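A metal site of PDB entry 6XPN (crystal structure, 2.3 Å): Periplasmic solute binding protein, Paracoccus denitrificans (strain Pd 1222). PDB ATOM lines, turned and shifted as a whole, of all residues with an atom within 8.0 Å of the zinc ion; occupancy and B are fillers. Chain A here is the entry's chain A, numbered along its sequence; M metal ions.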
ATOM      1  N   ASP A  59       7.241  15.280  20.821  1.00  0.00           N
ATOM      2  CA  ASP A  59       7.387  13.850  20.588  1.00  0.00           C
ATOM      3  C   ASP A  59       7.411  13.132  21.934  1.00  0.00           C
ATOM      4  O   ASP A  59       8.349  13.317  22.708  1.00  0.00           O
ATOM      5  CB  ASP A  59       8.691  13.588  19.826  1.00  0.00           C
ATOM      6  CG  ASP A  59       8.827  12.147  19.382  1.00  0.00           C
ATOM      7  OD1 ASP A  59       9.803  11.859  18.667  1.00  0.00           O
ATOM      8  OD2 ASP A  59       7.985  11.314  19.779  1.00  0.00           O
ATOM      9  N   THR A  60       6.396  12.316  22.192  1.00  0.00           N
ATOM     10  CA  THR A  60       6.349  11.597  23.464  1.00  0.00           C
ATOM     11  C   THR A  60       7.347  10.447  23.507  1.00  0.00           C
ATOM     12  O   THR A  60       7.869  10.128  24.575  1.00  0.00           O
ATOM     13  CB  THR A  60       4.920  11.110  23.710  1.00  0.00           C
ATOM     14  OG1 THR A  60       4.044  12.250  23.816  1.00  0.00           O
ATOM     15  CG2 THR A  60       4.838  10.273  24.983  1.00  0.00           C
ATOM     16  N   HIS A  61       7.653   9.841  22.346  1.00  0.00           N
ATOM     17  CA  HIS A  61       8.598   8.732  22.284  1.00  0.00           C
ATOM     18  C   HIS A  61       9.939   9.073  22.931  1.00  0.00           C
ATOM     19  O   HIS A  61      10.600   8.189  23.483  1.00  0.00           O
ATOM     20  CB  HIS A  61       8.842   8.322  20.825  1.00  0.00           C
ATOM     21  CG  HIS A  61       7.643   7.712  20.135  1.00  0.00           C
ATOM     22  ND1 HIS A  61       6.985   6.595  20.612  1.00  0.00           N
ATOM     23  CD2 HIS A  61       7.013   8.041  18.975  1.00  0.00           C
ATOM     24  CE1 HIS A  61       6.004   6.273  19.793  1.00  0.00           C
ATOM     25  NE2 HIS A  61       6.014   7.133  18.791  1.00  0.00           N
ATOM     26  N   PHE A  86       3.678   3.715  25.203  1.00  0.00           N
ATOM     27  CA  PHE A  86       3.846   4.994  24.528  1.00  0.00           C
ATOM     28  C   PHE A  86       4.652   5.960  25.387  1.00  0.00           C
ATOM     29  O   PHE A  86       5.624   6.575  24.922  1.00  0.00           O
ATOM     30  CB  PHE A  86       2.478   5.583  24.181  1.00  0.00           C
ATOM     31  CG  PHE A  86       2.544   6.844  23.382  1.00  0.00           C
ATOM     32  CD1 PHE A  86       3.242   6.880  22.202  1.00  0.00           C
ATOM     33  CD2 PHE A  86       1.871   7.990  23.802  1.00  0.00           C
ATOM     34  CE1 PHE A  86       3.309   8.060  21.440  1.00  0.00           C
ATOM     35  CE2 PHE A  86       1.921   9.163  23.052  1.00  0.00           C
ATOM     36  CZ  PHE A  86       2.641   9.196  21.875  1.00  0.00           C
ATOM     37  N   GLU A 115       3.034  -4.532  17.135  1.00  0.00           N
ATOM     38  CA  GLU A 115       3.969  -3.653  16.430  1.00  0.00           C
ATOM     39  C   GLU A 115       5.135  -4.355  15.737  1.00  0.00           C
ATOM     40  O   GLU A 115       6.170  -4.579  16.373  1.00  0.00           O
ATOM     41  CB  GLU A 115       4.507  -2.614  17.424  1.00  0.00           C
ATOM     42  CG  GLU A 115       5.503  -1.629  16.813  1.00  0.00           C
ATOM     43  CD  GLU A 115       5.297  -0.221  17.333  1.00  0.00           C
ATOM     44  OE1 GLU A 115       5.476   0.015  18.554  1.00  0.00           O
ATOM     45  OE2 GLU A 115       4.916   0.654  16.522  1.00  0.00           O
ATOM     46  N   ASP A 136       1.408  -1.763  18.998  1.00  0.00           N
ATOM     47  CA  ASP A 136       1.477  -0.425  18.381  1.00  0.00           C
ATOM     48  C   ASP A 136       0.679   0.548  19.237  1.00  0.00           C
ATOM     49  O   ASP A 136      -0.522   0.307  19.460  1.00  0.00           O
ATOM     50  CB  ASP A 136       0.954  -0.444  16.945  1.00  0.00           C
ATOM     51  CG  ASP A 136       1.242   0.862  16.185  1.00  0.00           C
ATOM     52  OD1 ASP A 136       1.305   1.938  16.801  1.00  0.00           O
ATOM     53  OD2 ASP A 136       1.417   0.810  14.945  1.00  0.00           O
ATOM     54  N   PRO A 137       1.290   1.601  19.787  1.00  0.00           N
ATOM     55  CA  PRO A 137       0.563   2.484  20.712  1.00  0.00           C
ATOM     56  C   PRO A 137      -0.370   3.491  20.059  1.00  0.00           C
ATOM     57  O   PRO A 137      -1.220   4.052  20.766  1.00  0.00           O
ATOM     58  CB  PRO A 137       1.696   3.233  21.424  1.00  0.00           C
ATOM     59  CG  PRO A 137       2.788   3.326  20.353  1.00  0.00           C
ATOM     60  CD  PRO A 137       2.686   2.022  19.574  1.00  0.00           C
ATOM     61  N   HIS A 138      -0.244   3.730  18.746  1.00  0.00           N
ATOM     62  CA  HIS A 138      -0.926   4.850  18.077  1.00  0.00           C
ATOM     63  C   HIS A 138      -2.402   4.577  17.762  1.00  0.00           C
ATOM     64  O   HIS A 138      -2.843   4.812  16.638  1.00  0.00           O
ATOM     65  CB  HIS A 138      -0.202   5.209  16.769  1.00  0.00           C
ATOM     66  CG  HIS A 138       1.269   5.444  16.916  1.00  0.00           C
ATOM     67  ND1 HIS A 138       2.205   4.431  16.832  1.00  0.00           N
ATOM     68  CD2 HIS A 138       1.967   6.592  17.117  1.00  0.00           C
ATOM     69  CE1 HIS A 138       3.417   4.947  16.983  1.00  0.00           C
ATOM     70  NE2 HIS A 138       3.301   6.249  17.138  1.00  0.00           N
ATOM     71  N   TRP A 140      -5.177   5.999  18.551  1.00  0.00           N
ATOM     72  CA  TRP A 140      -6.044   7.146  18.280  1.00  0.00           C
ATOM     73  C   TRP A 140      -6.164   7.474  16.787  1.00  0.00           C
ATOM     74  O   TRP A 140      -7.026   8.279  16.425  1.00  0.00           O
ATOM     75  CB  TRP A 140      -5.550   8.392  19.013  1.00  0.00           C
ATOM     76  CG  TRP A 140      -4.170   8.778  18.551  1.00  0.00           C
ATOM     77  CD1 TRP A 140      -3.859   9.517  17.433  1.00  0.00           C
ATOM     78  CD2 TRP A 140      -2.926   8.437  19.165  1.00  0.00           C
ATOM     79  NE1 TRP A 140      -2.497   9.647  17.333  1.00  0.00           N
ATOM     80  CE2 TRP A 140      -1.902   8.991  18.377  1.00  0.00           C
ATOM     81  CE3 TRP A 140      -2.586   7.699  20.307  1.00  0.00           C
ATOM     82  CZ2 TRP A 140      -0.555   8.837  18.681  1.00  0.00           C
ATOM     83  CZ3 TRP A 140      -1.251   7.550  20.606  1.00  0.00           C
ATOM     84  CH2 TRP A 140      -0.254   8.116  19.798  1.00  0.00           C
ATOM     85  N   HIS A 204       7.264   8.765  10.390  1.00  0.00           N
ATOM     86  CA  HIS A 204       7.435   7.484  11.083  1.00  0.00           C
ATOM     87  C   HIS A 204       6.134   6.670  11.036  1.00  0.00           C
ATOM     88  O   HIS A 204       5.085   7.125  10.559  1.00  0.00           O
ATOM     89  CB  HIS A 204       7.979   7.663  12.525  1.00  0.00           C
ATOM     90  CG  HIS A 204       6.965   8.066  13.569  1.00  0.00           C
ATOM     91  ND1 HIS A 204       6.364   9.307  13.582  1.00  0.00           N
ATOM     92  CD2 HIS A 204       6.546   7.432  14.689  1.00  0.00           C
ATOM     93  CE1 HIS A 204       5.578   9.391  14.646  1.00  0.00           C
ATOM     94  NE2 HIS A 204       5.671   8.277  15.335  1.00  0.00           N
ATOM     95  N   ASN A 205       6.268   5.423  11.482  1.00  0.00           N
ATOM     96  CA  ASN A 205       5.223   4.396  11.376  1.00  0.00           C
ATOM     97  C   ASN A 205       4.152   4.613  12.458  1.00  0.00           C
ATOM     98  O   ASN A 205       3.946   3.790  13.366  1.00  0.00           O
ATOM     99  CB  ASN A 205       5.868   3.024  11.462  1.00  0.00           C
ATOM    100  CG  ASN A 205       5.033   1.940  10.834  1.00  0.00           C
ATOM    101  OD1 ASN A 205       4.012   2.211  10.197  1.00  0.00           O
ATOM    102  ND2 ASN A 205       5.474   0.701  10.973  1.00  0.00           N
ATOM    103  N   ALA A 206       3.428   5.723  12.323  1.00  0.00           N
ATOM    104  CA  ALA A 206       2.454   6.148  13.331  1.00  0.00           C
ATOM    105  C   ALA A 206       0.992   5.998  12.891  1.00  0.00           C
ATOM    106  O   ALA A 206       0.106   6.395  13.655  1.00  0.00           O
ATOM    107  CB  ALA A 206       2.718   7.597  13.717  1.00  0.00           C
ATOM    108  N   PHE A 207       0.720   5.449  11.704  1.00  0.00           N
ATOM    109  CA  PHE A 207      -0.595   5.505  11.097  1.00  0.00           C
ATOM    110  C   PHE A 207      -1.144   4.125  10.776  1.00  0.00           C
ATOM    111  O   PHE A 207      -2.069   3.999   9.962  1.00  0.00           O
ATOM    112  CB  PHE A 207      -0.570   6.341   9.807  1.00  0.00           C
ATOM    113  CG  PHE A 207      -0.285   7.796  10.031  1.00  0.00           C
ATOM    114  CD1 PHE A 207      -1.332   8.702  10.234  1.00  0.00           C
ATOM    115  CD2 PHE A 207       1.023   8.270  10.038  1.00  0.00           C
ATOM    116  CE1 PHE A 207      -1.068  10.060  10.443  1.00  0.00           C
ATOM    117  CE2 PHE A 207       1.283   9.625  10.233  1.00  0.00           C
ATOM    118  CZ  PHE A 207       0.237  10.523  10.431  1.00  0.00           C
ATOM    119  N   GLU A 245       5.930  15.641   9.328  1.00  0.00           N
ATOM    120  CA  GLU A 245       5.170  15.472  10.557  1.00  0.00           C
ATOM    121  C   GLU A 245       5.470  16.654  11.476  1.00  0.00           C
ATOM    122  O   GLU A 245       6.612  17.135  11.532  1.00  0.00           O
ATOM    123  CB  GLU A 245       5.547  14.171  11.279  1.00  0.00           C
ATOM    124  CG  GLU A 245       4.773  12.942  10.810  1.00  0.00           C
ATOM    125  CD  GLU A 245       5.199  11.673  11.535  1.00  0.00           C
ATOM    126  OE1 GLU A 245       5.098  10.583  10.923  1.00  0.00           O
ATOM    127  OE2 GLU A 245       5.673  11.778  12.697  1.00  0.00           O
ATOM    128  N   ILE A 247       5.815  16.704  14.665  1.00  0.00           N
ATOM    129  CA  ILE A 247       6.577  16.429  15.887  1.00  0.00           C
ATOM    130  C   ILE A 247       8.079  16.324  15.631  1.00  0.00           C
ATOM    131  O   ILE A 247       8.856  16.299  16.599  1.00  0.00           O
ATOM    132  CB  ILE A 247       6.080  15.138  16.569  1.00  0.00           C
ATOM    133  CG1 ILE A 247       6.306  13.914  15.691  1.00  0.00           C
ATOM    134  CG2 ILE A 247       4.577  15.278  16.883  1.00  0.00           C
ATOM    135  CD1 ILE A 247       6.316  12.549  16.448  1.00  0.00           C
ATOM    136  N   SER A 270       0.745  13.563  13.656  1.00  0.00           N
ATOM    137  CA  SER A 270       0.801  12.159  14.033  1.00  0.00           C
ATOM    138  C   SER A 270       0.551  11.950  15.529  1.00  0.00           C
ATOM    139  O   SER A 270      -0.480  11.379  15.906  1.00  0.00           O
ATOM    140  CB  SER A 270       2.154  11.570  13.652  1.00  0.00           C
ATOM    141  OG  SER A 270       3.212  12.357  14.168  1.00  0.00           O
ATOM    142  N   ASP A 271       1.489  12.370  16.398  1.00  0.00           N
ATOM    143  CA  ASP A 271       1.456  12.032  17.814  1.00  0.00           C
ATOM    144  C   ASP A 271       1.185  13.235  18.707  1.00  0.00           C
ATOM    145  O   ASP A 271       1.338  13.142  19.930  1.00  0.00           O
ATOM    146  CB  ASP A 271       2.768  11.383  18.278  1.00  0.00           C
ATOM    147  CG  ASP A 271       3.037  10.033  17.625  1.00  0.00           C
ATOM    148  OD1 ASP A 271       4.019   9.368  18.044  1.00  0.00           O
ATOM    149  OD2 ASP A 271       2.308   9.648  16.695  1.00  0.00           O
ATOM    150  N   ALA A 272       0.855  14.386  18.134  1.00  0.00           N
ATOM    151  CA  ALA A 272       0.604  15.595  18.902  1.00  0.00           C
ATOM    152  C   ALA A 272      -0.282  16.511  18.091  1.00  0.00           C
ATOM    153  O   ALA A 272      -0.212  16.541  16.852  1.00  0.00           O
ATOM    154  CB  ALA A 272       1.910  16.307  19.288  1.00  0.00           C
HETATM  155 ZN    ZN M   1       4.700   7.732  17.296  1.00  0.00          ZN
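The zinc ion is bound by OD1 of Asp 271 (1.9 Å). The zinc ion is bound by NE2 of His 138 (2.0 Å). A ring nitrogen (NE2) of His 61 binds the zinc ion. NE2 of His 204 binds the zinc ion (2.3 Å).
The backbone NH (N) of His 61 is in hydrogen-bond range of the side-chain carboxylate (OD2) of Asp 59 (3.0 Å). ND1 of His 204 lies within hydrogen-bond range of OE2 of Glu 245, at 2.7 Å. A ring nitrogen (ND1) of His 138 lies within hydrogen-bond range of the side-chain carboxylate (OD1) of Asp 136, at 2.7 Å.
Of the 18 residues printed, 4 come within 4 Å of the zinc ion.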
